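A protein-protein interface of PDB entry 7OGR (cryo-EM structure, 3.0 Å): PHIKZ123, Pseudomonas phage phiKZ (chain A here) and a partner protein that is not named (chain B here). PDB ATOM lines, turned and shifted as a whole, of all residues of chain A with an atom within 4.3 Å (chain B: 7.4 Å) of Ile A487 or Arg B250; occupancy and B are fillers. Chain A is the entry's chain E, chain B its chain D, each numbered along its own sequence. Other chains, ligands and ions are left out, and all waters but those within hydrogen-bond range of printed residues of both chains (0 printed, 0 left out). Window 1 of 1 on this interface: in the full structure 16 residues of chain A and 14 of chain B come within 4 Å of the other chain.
The backbone carbonyl oxygen of Ser B249 lies within hydrogen-bond range of the side-chain amide nitrogen of Gln A500 (2.9 Å).
The backbone carbonyl oxygen of Asp A506 sits at hydrogen-bond distance from the guanidinium group of Arg B250 (2.8 Å).
OE1 of Gln A500 sits at hydrogen-bond distance from OG1 of Thr B253 (2.8 Å).
NZ of Lys B254 sits close to NE2 of Gln A500, at 3.3 Å.
The side-chain amino group (NZ) of Lys B254 lies within hydrogen-bond range of the backbone carbonyl oxygen (O) of Pro A505, 2.4 Å away.
O of Phe B227 sits at hydrogen-bond distance from OH of Tyr B243 (2.8 Å).
The backbone carbonyl oxygen (O) of Met B246 sits at hydrogen-bond distance from the side-chain hydroxyl (OG) of Ser B249 (2.6 Å).
The backbone carbonyl oxygen of Ser B249 sits close to the side-chain amino group of Lys B254 (3.5 Å).
The backbone carbonyl oxygen of Ile A487 lies within hydrogen-bond range of the guanidinium group of Arg A541 (3.1 Å).
Of chain B, only Asp B221 (3.9 Å), Phe B227 (3.7 Å), Met B246 (3.9 Å) and Arg B250 (3.6 Å) come within 4 Å of Ile A487.
Arg B250 touches just these residues of chain A: Ile A487 (3.6 Å), Gln A500 (3.8 Å), Asp A506 (2.8 Å) and Gly A507 (3.9 Å).
Printed residues of chain B within 4 Å of Pro A505: Lys B254.
Printed residues of chain A within 4 Å of Ser B249: Gln A500.
Printed residues of chain A within 4 Å of Lys B254: Gln A500 and Pro A505.
Printed residues of chain B that touch a printed residue of chain A: Asp B221, Phe B227, Tyr B243, Met B246, Ser B249, Arg B250, Thr B253 and Lys B254.
Printed residues of chain A that touch a printed residue of chain B: Ile A486, Ile A487, His A488, Gln A500, Pro A505, Asp A506, Gly A507 and Phe A540.
Among the printed residues, no Asp or Glu carboxylate lies within 4 Å of a Lys or Arg side-chain nitrogen of the other chain.
CA of Ile A486 touches OD2 of Asp B221 (3.9 Å).
Asp B221 touches Ile A487.
Ile A487 touches Phe B227 (CG2 to CE2, 3.7 Å).
Ile A487 touches Met B246 (CD1 to O, 3.9 Å).
NH2 of Arg B250 touches CG1 of Ile A487, 3.6 Å away.
His A488 touches Met B246 (O to CE, 3.3 Å).
Arg B250 touches Gln A500 (NH1 to NE2, 3.8 Å).
Arg B250 touches Gly A507.
CD1 of Tyr B243 touches CE1 of Phe A540, 3.5 Å away.
Phe A540 touches Met B246.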
ATOM      1  N   THR A 380      -7.867  40.379  21.217  1.00  0.00           N
ATOM      2  CA  THR A 380      -7.471  39.299  22.115  1.00  0.00           C
ATOM      3  C   THR A 380      -5.955  39.205  22.228  1.00  0.00           C
ATOM      4  O   THR A 380      -5.432  38.178  22.672  1.00  0.00           O
ATOM      5  CB  THR A 380      -8.036  37.949  21.655  1.00  0.00           C
ATOM      6  OG1 THR A 380      -7.537  37.639  20.348  1.00  0.00           O
ATOM      7  CG2 THR A 380      -9.559  37.955  21.630  1.00  0.00           C
ATOM      8  N   ILE A 486     -10.437  34.538  23.799  1.00  0.00           N
ATOM      9  CA  ILE A 486     -10.216  33.644  22.677  1.00  0.00           C
ATOM     10  C   ILE A 486      -8.714  33.392  22.589  1.00  0.00           C
ATOM     11  O   ILE A 486      -7.905  34.103  23.192  1.00  0.00           O
ATOM     12  CB  ILE A 486     -10.784  34.243  21.365  1.00  0.00           C
ATOM     13  CG1 ILE A 486     -12.081  34.995  21.651  1.00  0.00           C
ATOM     14  CG2 ILE A 486     -11.136  33.157  20.351  1.00  0.00           C
ATOM     15  CD1 ILE A 486     -12.586  35.803  20.476  1.00  0.00           C
ATOM     16  N   ILE A 487      -8.333  32.343  21.853  1.00  0.00           N
ATOM     17  CA  ILE A 487      -6.927  31.991  21.702  1.00  0.00           C
ATOM     18  C   ILE A 487      -6.202  33.053  20.877  1.00  0.00           C
ATOM     19  O   ILE A 487      -6.808  33.793  20.085  1.00  0.00           O
ATOM     20  CB  ILE A 487      -6.790  30.584  21.081  1.00  0.00           C
ATOM     21  CG1 ILE A 487      -5.487  29.908  21.524  1.00  0.00           C
ATOM     22  CG2 ILE A 487      -6.901  30.612  19.555  1.00  0.00           C
ATOM     23  CD1 ILE A 487      -5.289  28.523  20.945  1.00  0.00           C
ATOM     24  N   HIS A 488      -4.898  33.169  21.115  1.00  0.00           N
ATOM     25  CA  HIS A 488      -4.022  34.091  20.408  1.00  0.00           C
ATOM     26  C   HIS A 488      -2.595  33.609  20.608  1.00  0.00           C
ATOM     27  O   HIS A 488      -2.270  33.018  21.640  1.00  0.00           O
ATOM     28  CB  HIS A 488      -4.177  35.532  20.913  1.00  0.00           C
ATOM     29  CG  HIS A 488      -3.819  36.573  19.897  1.00  0.00           C
ATOM     30  ND1 HIS A 488      -2.525  36.798  19.485  1.00  0.00           N
ATOM     31  CD2 HIS A 488      -4.590  37.448  19.210  1.00  0.00           C
ATOM     32  CE1 HIS A 488      -2.511  37.767  18.587  1.00  0.00           C
ATOM     33  NE2 HIS A 488      -3.752  38.179  18.402  1.00  0.00           N
ATOM     34  N   ILE A 491      -0.305  35.029  23.600  1.00  0.00           N
ATOM     35  CA  ILE A 491      -0.286  34.375  24.901  1.00  0.00           C
ATOM     36  C   ILE A 491       0.949  33.493  25.068  1.00  0.00           C
ATOM     37  O   ILE A 491       1.396  33.261  26.195  1.00  0.00           O
ATOM     38  CB  ILE A 491      -1.593  33.579  25.087  1.00  0.00           C
ATOM     39  CG1 ILE A 491      -2.781  34.397  24.580  1.00  0.00           C
ATOM     40  CG2 ILE A 491      -1.824  33.238  26.539  1.00  0.00           C
ATOM     41  CD1 ILE A 491      -4.095  33.647  24.599  1.00  0.00           C
ATOM     42  N   GLN A 500      -2.951  27.854  34.257  1.00  0.00           N
ATOM     43  CA  GLN A 500      -4.371  28.157  34.100  1.00  0.00           C
ATOM     44  C   GLN A 500      -5.080  28.084  35.448  1.00  0.00           C
ATOM     45  O   GLN A 500      -5.615  27.032  35.823  1.00  0.00           O
ATOM     46  CB  GLN A 500      -4.991  27.203  33.081  1.00  0.00           C
ATOM     47  CG  GLN A 500      -4.445  27.415  31.669  1.00  0.00           C
ATOM     48  CD  GLN A 500      -4.542  26.189  30.787  1.00  0.00           C
ATOM     49  OE1 GLN A 500      -4.840  25.096  31.255  1.00  0.00           O
ATOM     50  NE2 GLN A 500      -4.289  26.370  29.498  1.00  0.00           N
ATOM     51  N   PRO A 505      -8.049  31.787  33.408  1.00  0.00           N
ATOM     52  CA  PRO A 505      -7.635  30.505  32.826  1.00  0.00           C
ATOM     53  C   PRO A 505      -7.263  30.548  31.352  1.00  0.00           C
ATOM     54  O   PRO A 505      -6.851  29.515  30.817  1.00  0.00           O
ATOM     55  CB  PRO A 505      -8.886  29.646  33.036  1.00  0.00           C
ATOM     56  CG  PRO A 505     -10.017  30.614  32.893  1.00  0.00           C
ATOM     57  CD  PRO A 505      -9.510  31.975  33.319  1.00  0.00           C
ATOM     58  N   ASP A 506      -7.374  31.694  30.686  1.00  0.00           N
ATOM     59  CA  ASP A 506      -7.093  31.774  29.259  1.00  0.00           C
ATOM     60  C   ASP A 506      -5.618  31.982  28.947  1.00  0.00           C
ATOM     61  O   ASP A 506      -5.251  32.021  27.767  1.00  0.00           O
ATOM     62  CB  ASP A 506      -7.919  32.897  28.619  1.00  0.00           C
ATOM     63  CG  ASP A 506      -7.778  34.221  29.348  1.00  0.00           C
ATOM     64  OD1 ASP A 506      -7.129  34.262  30.415  1.00  0.00           O
ATOM     65  OD2 ASP A 506      -8.322  35.229  28.852  1.00  0.00           O
ATOM     66  N   GLY A 507      -4.770  32.119  29.962  1.00  0.00           N
ATOM     67  CA  GLY A 507      -3.359  32.359  29.757  1.00  0.00           C
ATOM     68  C   GLY A 507      -2.927  33.792  29.964  1.00  0.00           C
ATOM     69  O   GLY A 507      -1.732  34.085  29.835  1.00  0.00           O
ATOM     70  N   PHE A 540      -4.547  29.854  13.675  1.00  0.00           N
ATOM     71  CA  PHE A 540      -5.610  29.877  14.685  1.00  0.00           C
ATOM     72  C   PHE A 540      -6.977  30.295  14.156  1.00  0.00           C
ATOM     73  O   PHE A 540      -7.865  30.581  14.952  1.00  0.00           O
ATOM     74  CB  PHE A 540      -5.249  30.821  15.838  1.00  0.00           C
ATOM     75  CG  PHE A 540      -4.288  30.243  16.841  1.00  0.00           C
ATOM     76  CD1 PHE A 540      -4.052  28.878  16.911  1.00  0.00           C
ATOM     77  CD2 PHE A 540      -3.623  31.078  17.728  1.00  0.00           C
ATOM     78  CE1 PHE A 540      -3.168  28.361  17.846  1.00  0.00           C
ATOM     79  CE2 PHE A 540      -2.738  30.566  18.660  1.00  0.00           C
ATOM     80  CZ  PHE A 540      -2.510  29.207  18.716  1.00  0.00           C
ATOM     81  N   ARG A 541      -7.039  30.809  12.891  1.00  0.00           N
ATOM     82  CA  ARG A 541      -8.094  31.756  12.397  1.00  0.00           C
ATOM     83  C   ARG A 541      -8.388  31.390  10.940  1.00  0.00           C
ATOM     84  O   ARG A 541      -7.793  31.954  10.017  1.00  0.00           O
ATOM     85  CB  ARG A 541      -7.664  33.216  12.526  1.00  0.00           C
ATOM     86  CG  ARG A 541      -7.436  33.722  13.948  1.00  0.00           C
ATOM     87  CD  ARG A 541      -8.704  34.306  14.553  1.00  0.00           C
ATOM     88  NE  ARG A 541      -8.417  35.202  15.671  1.00  0.00           N
ATOM     89  CZ  ARG A 541      -8.225  34.802  16.925  1.00  0.00           C
ATOM     90  NH1 ARG A 541      -7.968  35.693  17.873  1.00  0.00           N
ATOM     91  NH2 ARG A 541      -8.293  33.514  17.235  1.00  0.00           N
ATOM     92  N   ARG B 216      -5.428  12.512  18.655  1.00  0.00           N
ATOM     93  CA  ARG B 216      -6.420  13.387  19.257  1.00  0.00           C
ATOM     94  C   ARG B 216      -7.031  14.266  18.170  1.00  0.00           C
ATOM     95  O   ARG B 216      -6.343  14.717  17.250  1.00  0.00           O
ATOM     96  CB  ARG B 216      -5.786  14.243  20.356  1.00  0.00           C
ATOM     97  CG  ARG B 216      -6.772  15.055  21.184  1.00  0.00           C
ATOM     98  CD  ARG B 216      -6.073  15.810  22.302  1.00  0.00           C
ATOM     99  NE  ARG B 216      -6.983  16.715  23.000  1.00  0.00           N
ATOM    100  CZ  ARG B 216      -7.743  16.365  24.032  1.00  0.00           C
ATOM    101  NH1 ARG B 216      -8.541  17.257  24.602  1.00  0.00           N
ATOM    102  NH2 ARG B 216      -7.702  15.125  24.498  1.00  0.00           N
ATOM    103  N   PRO B 219     -10.014  19.746  19.199  1.00  0.00           N
ATOM    104  CA  PRO B 219     -10.483  20.305  20.469  1.00  0.00           C
ATOM    105  C   PRO B 219     -11.145  21.664  20.262  1.00  0.00           C
ATOM    106  O   PRO B 219     -11.010  22.305  19.220  1.00  0.00           O
ATOM    107  CB  PRO B 219      -9.198  20.428  21.297  1.00  0.00           C
ATOM    108  CG  PRO B 219      -8.157  19.634  20.551  1.00  0.00           C
ATOM    109  CD  PRO B 219      -8.545  19.778  19.122  1.00  0.00           C
ATOM    110  N   THR B 220     -11.874  22.096  21.288  1.00  0.00           N
ATOM    111  CA  THR B 220     -12.680  23.304  21.210  1.00  0.00           C
ATOM    112  C   THR B 220     -12.037  24.449  21.996  1.00  0.00           C
ATOM    113  O   THR B 220     -10.911  24.351  22.491  1.00  0.00           O
ATOM    114  CB  THR B 220     -14.101  23.023  21.706  1.00  0.00           C
ATOM    115  OG1 THR B 220     -14.106  22.957  23.137  1.00  0.00           O
ATOM    116  CG2 THR B 220     -14.613  21.708  21.138  1.00  0.00           C
ATOM    117  N   ASP B 221     -12.769  25.554  22.102  1.00  0.00           N
ATOM    118  CA  ASP B 221     -12.374  26.781  22.780  1.00  0.00           C
ATOM    119  C   ASP B 221     -13.380  27.043  23.907  1.00  0.00           C
ATOM    120  O   ASP B 221     -14.094  26.133  24.339  1.00  0.00           O
ATOM    121  CB  ASP B 221     -12.283  27.935  21.774  1.00  0.00           C
ATOM    122  CG  ASP B 221     -11.298  29.014  22.199  1.00  0.00           C
ATOM    123  OD1 ASP B 221     -10.075  28.781  22.099  1.00  0.00           O
ATOM    124  OD2 ASP B 221     -11.751  30.095  22.632  1.00  0.00           O
ATOM    125  N   ILE B 222     -13.381  28.280  24.424  1.00  0.00           N
ATOM    126  CA  ILE B 222     -14.387  28.724  25.393  1.00  0.00           C
ATOM    127  C   ILE B 222     -15.796  28.566  24.834  1.00  0.00           C
ATOM    128  O   ILE B 222     -16.706  28.103  25.535  1.00  0.00           O
ATOM    129  CB  ILE B 222     -14.102  30.186  25.800  1.00  0.00           C
ATOM    130  CG1 ILE B 222     -12.750  30.294  26.499  1.00  0.00           C
ATOM    131  CG2 ILE B 222     -15.201  30.739  26.702  1.00  0.00           C
ATOM    132  CD1 ILE B 222     -12.702  29.546  27.801  1.00  0.00           C
ATOM    133  N   PHE B 227     -11.027  23.923  15.185  1.00  0.00           N
ATOM    134  CA  PHE B 227      -9.891  24.741  14.784  1.00  0.00           C
ATOM    135  C   PHE B 227      -9.357  24.380  13.404  1.00  0.00           C
ATOM    136  O   PHE B 227      -8.241  24.795  13.063  1.00  0.00           O
ATOM    137  CB  PHE B 227      -8.772  24.628  15.822  1.00  0.00           C
ATOM    138  CG  PHE B 227      -8.935  25.556  16.988  1.00  0.00           C
ATOM    139  CD1 PHE B 227      -9.681  25.175  18.093  1.00  0.00           C
ATOM    140  CD2 PHE B 227      -8.350  26.812  16.977  1.00  0.00           C
ATOM    141  CE1 PHE B 227      -9.838  26.028  19.169  1.00  0.00           C
ATOM    142  CE2 PHE B 227      -8.502  27.671  18.050  1.00  0.00           C
ATOM    143  CZ  PHE B 227      -9.248  27.278  19.147  1.00  0.00           C
ATOM    144  N   LEU B 242       3.584  24.238  18.843  1.00  0.00           N
ATOM    145  CA  LEU B 242       2.943  25.350  19.544  1.00  0.00           C
ATOM    146  C   LEU B 242       1.440  25.380  19.295  1.00  0.00           C
ATOM    147  O   LEU B 242       0.661  25.629  20.225  1.00  0.00           O
ATOM    148  CB  LEU B 242       3.576  26.674  19.115  1.00  0.00           C
ATOM    149  CG  LEU B 242       3.114  27.938  19.845  1.00  0.00           C
ATOM    150  CD1 LEU B 242       3.296  27.802  21.347  1.00  0.00           C
ATOM    151  CD2 LEU B 242       3.848  29.162  19.325  1.00  0.00           C
ATOM    152  N   TYR B 243       1.024  25.035  18.078  1.00  0.00           N
ATOM    153  CA  TYR B 243      -0.371  25.104  17.656  1.00  0.00           C
ATOM    154  C   TYR B 243      -1.228  24.077  18.392  1.00  0.00           C
ATOM    155  O   TYR B 243      -2.200  24.430  19.075  1.00  0.00           O
ATOM    156  CB  TYR B 243      -0.425  24.887  16.139  1.00  0.00           C
ATOM    157  CG  TYR B 243      -1.798  24.806  15.522  1.00  0.00           C
ATOM    158  CD1 TYR B 243      -2.617  25.920  15.461  1.00  0.00           C
ATOM    159  CD2 TYR B 243      -2.261  23.617  14.969  1.00  0.00           C
ATOM    160  CE1 TYR B 243      -3.867  25.854  14.890  1.00  0.00           C
ATOM    161  CE2 TYR B 243      -3.513  23.540  14.390  1.00  0.00           C
ATOM    162  CZ  TYR B 243      -4.308  24.665  14.348  1.00  0.00           C
ATOM    163  OH  TYR B 243      -5.560  24.604  13.781  1.00  0.00           O
ATOM    164  N   GLU B 244      -0.839  22.803  18.301  1.00  0.00           N
ATOM    165  CA  GLU B 244      -1.644  21.724  18.860  1.00  0.00           C
ATOM    166  C   GLU B 244      -1.607  21.728  20.386  1.00  0.00           C
ATOM    167  O   GLU B 244      -2.619  21.434  21.035  1.00  0.00           O
ATOM    168  CB  GLU B 244      -1.156  20.389  18.302  1.00  0.00           C
ATOM    169  CG  GLU B 244      -1.166  20.314  16.782  1.00  0.00           C
ATOM    170  CD  GLU B 244      -0.405  19.114  16.249  1.00  0.00           C
ATOM    171  OE1 GLU B 244      -0.048  18.226  17.051  1.00  0.00           O
ATOM    172  OE2 GLU B 244      -0.159  19.062  15.026  1.00  0.00           O
ATOM    173  N   ASN B 245      -0.463  22.091  20.978  1.00  0.00           N
ATOM    174  CA  ASN B 245      -0.397  22.189  22.433  1.00  0.00           C
ATOM    175  C   ASN B 245      -1.174  23.388  22.954  1.00  0.00           C
ATOM    176  O   ASN B 245      -1.748  23.314  24.045  1.00  0.00           O
ATOM    177  CB  ASN B 245       1.053  22.259  22.913  1.00  0.00           C
ATOM    178  CG  ASN B 245       1.258  21.590  24.257  1.00  0.00           C
ATOM    179  OD1 ASN B 245       0.320  21.425  25.034  1.00  0.00           O
ATOM    180  ND2 ASN B 245       2.494  21.195  24.534  1.00  0.00           N
ATOM    181  N   MET B 246      -1.251  24.484  22.191  1.00  0.00           N
ATOM    182  CA  MET B 246      -2.098  25.583  22.645  1.00  0.00           C
ATOM    183  C   MET B 246      -3.581  25.249  22.523  1.00  0.00           C
ATOM    184  O   MET B 246      -4.372  25.646  23.388  1.00  0.00           O
ATOM    185  CB  MET B 246      -1.774  26.866  21.878  1.00  0.00           C
ATOM    186  CG  MET B 246      -0.599  27.639  22.456  1.00  0.00           C
ATOM    187  SD  MET B 246      -0.577  29.366  21.951  1.00  0.00           S
ATOM    188  CE  MET B 246      -1.887  30.009  22.986  1.00  0.00           C
ATOM    189  N   ILE B 247      -3.969  24.470  21.507  1.00  0.00           N
ATOM    190  CA  ILE B 247      -5.373  24.067  21.405  1.00  0.00           C
ATOM    191  C   ILE B 247      -5.733  23.068  22.507  1.00  0.00           C
ATOM    192  O   ILE B 247      -6.820  23.138  23.100  1.00  0.00           O
ATOM    193  CB  ILE B 247      -5.678  23.515  20.002  1.00  0.00           C
ATOM    194  CG1 ILE B 247      -5.416  24.577  18.947  1.00  0.00           C
ATOM    195  CG2 ILE B 247      -7.132  23.139  19.871  1.00  0.00           C
ATOM    196  CD1 ILE B 247      -5.513  24.041  17.560  1.00  0.00           C
ATOM    197  N   GLU B 248      -4.819  22.143  22.828  1.00  0.00           N
ATOM    198  CA  GLU B 248      -5.081  21.242  23.949  1.00  0.00           C
ATOM    199  C   GLU B 248      -5.045  21.983  25.286  1.00  0.00           C
ATOM    200  O   GLU B 248      -5.720  21.572  26.236  1.00  0.00           O
ATOM    201  CB  GLU B 248      -4.107  20.056  23.941  1.00  0.00           C
ATOM    202  CG  GLU B 248      -2.776  20.267  24.645  1.00  0.00           C
ATOM    203  CD  GLU B 248      -1.948  19.009  24.713  1.00  0.00           C
ATOM    204  OE1 GLU B 248      -1.305  18.764  25.754  1.00  0.00           O
ATOM    205  OE2 GLU B 248      -1.943  18.261  23.718  1.00  0.00           O
ATOM    206  N   SER B 249      -4.295  23.089  25.371  1.00  0.00           N
ATOM    207  CA  SER B 249      -4.340  23.922  26.566  1.00  0.00           C
ATOM    208  C   SER B 249      -5.679  24.631  26.696  1.00  0.00           C
ATOM    209  O   SER B 249      -6.163  24.839  27.814  1.00  0.00           O
ATOM    210  CB  SER B 249      -3.199  24.940  26.543  1.00  0.00           C
ATOM    211  OG  SER B 249      -3.551  26.085  25.788  1.00  0.00           O
ATOM    212  N   ARG B 250      -6.299  24.998  25.573  1.00  0.00           N
ATOM    213  CA  ARG B 250      -7.654  25.536  25.653  1.00  0.00           C
ATOM    214  C   ARG B 250      -8.700  24.465  25.929  1.00  0.00           C
ATOM    215  O   ARG B 250      -9.767  24.787  26.462  1.00  0.00           O
ATOM    216  CB  ARG B 250      -8.034  26.291  24.378  1.00  0.00           C
ATOM    217  CG  ARG B 250      -7.050  27.354  23.971  1.00  0.00           C
ATOM    218  CD  ARG B 250      -7.375  28.692  24.617  1.00  0.00           C
ATOM    219  NE  ARG B 250      -6.700  28.851  25.903  1.00  0.00           N
ATOM    220  CZ  ARG B 250      -5.430  29.218  26.048  1.00  0.00           C
ATOM    221  NH1 ARG B 250      -4.909  29.327  27.261  1.00  0.00           N
ATOM    222  NH2 ARG B 250      -4.682  29.490  24.988  1.00  0.00           N
ATOM    223  N   SER B 251      -8.427  23.207  25.582  1.00  0.00           N
ATOM    224  CA  SER B 251      -9.402  22.155  25.853  1.00  0.00           C
ATOM    225  C   SER B 251      -9.306  21.586  27.263  1.00  0.00           C
ATOM    226  O   SER B 251     -10.320  21.118  27.793  1.00  0.00           O
ATOM    227  CB  SER B 251      -9.247  21.005  24.863  1.00  0.00           C
ATOM    228  OG  SER B 251      -8.055  20.284  25.098  1.00  0.00           O
ATOM    229  N   GLY B 252      -8.123  21.608  27.876  1.00  0.00           N
ATOM    230  CA  GLY B 252      -7.899  20.884  29.113  1.00  0.00           C
ATOM    231  C   GLY B 252      -8.593  21.400  30.357  1.00  0.00           C
ATOM    232  O   GLY B 252      -9.356  20.667  30.992  1.00  0.00           O
ATOM    233  N   THR B 253      -8.340  22.654  30.723  1.00  0.00           N
ATOM    234  CA  THR B 253      -8.748  23.178  32.022  1.00  0.00           C
ATOM    235  C   THR B 253     -10.039  23.988  31.965  1.00  0.00           C
ATOM    236  O   THR B 253     -10.888  23.849  32.855  1.00  0.00           O
ATOM    237  CB  THR B 253      -7.614  24.037  32.599  1.00  0.00           C
ATOM    238  OG1 THR B 253      -6.430  23.236  32.712  1.00  0.00           O
ATOM    239  CG2 THR B 253      -7.954  24.585  33.977  1.00  0.00           C
ATOM    240  N   LYS B 254     -10.210  24.811  30.923  1.00  0.00           N
ATOM    241  CA  LYS B 254     -11.347  25.727  30.847  1.00  0.00           C
ATOM    242  C   LYS B 254     -12.670  25.002  30.650  1.00  0.00           C
ATOM    243  O   LYS B 254     -13.723  25.531  31.027  1.00  0.00           O
ATOM    244  CB  LYS B 254     -11.127  26.731  29.722  1.00  0.00           C
ATOM    245  CG  LYS B 254     -10.272  27.910  30.120  1.00  0.00           C
ATOM    246  CD  LYS B 254      -9.401  28.367  28.976  1.00  0.00           C
ATOM    247  CE  LYS B 254      -8.277  27.388  28.746  1.00  0.00           C
ATOM    248  NZ  LYS B 254      -7.393  27.311  29.927  1.00  0.00           N
ATOM    249  N   ALA B 255     -12.645  23.810  30.056  1.00  0.00           N
ATOM    250  CA  ALA B 255     -13.861  23.012  29.958  1.00  0.00           C
ATOM    251  C   ALA B 255     -14.268  22.472  31.322  1.00  0.00           C
ATOM    252  O   ALA B 255     -15.440  22.541  31.705  1.00  0.00           O
ATOM    253  CB  ALA B 255     -13.661  21.870  28.960  1.00  0.00           C
ATOM    254  N   LEU B 256     -13.301  21.947  32.079  1.00  0.00           N
ATOM    255  CA  LEU B 256     -13.611  21.334  33.366  1.00  0.00           C
ATOM    256  C   LEU B 256     -13.967  22.375  34.423  1.00  0.00           C
ATOM    257  O   LEU B 256     -14.745  22.082  35.337  1.00  0.00           O
ATOM    258  CB  LEU B 256     -12.433  20.477  33.830  1.00  0.00           C
ATOM    259  CG  LEU B 256     -12.779  19.250  34.676  1.00  0.00           C
ATOM    260  CD1 LEU B 256     -13.674  18.307  33.897  1.00  0.00           C
ATOM    261  CD2 LEU B 256     -11.514  18.541  35.127  1.00  0.00           C
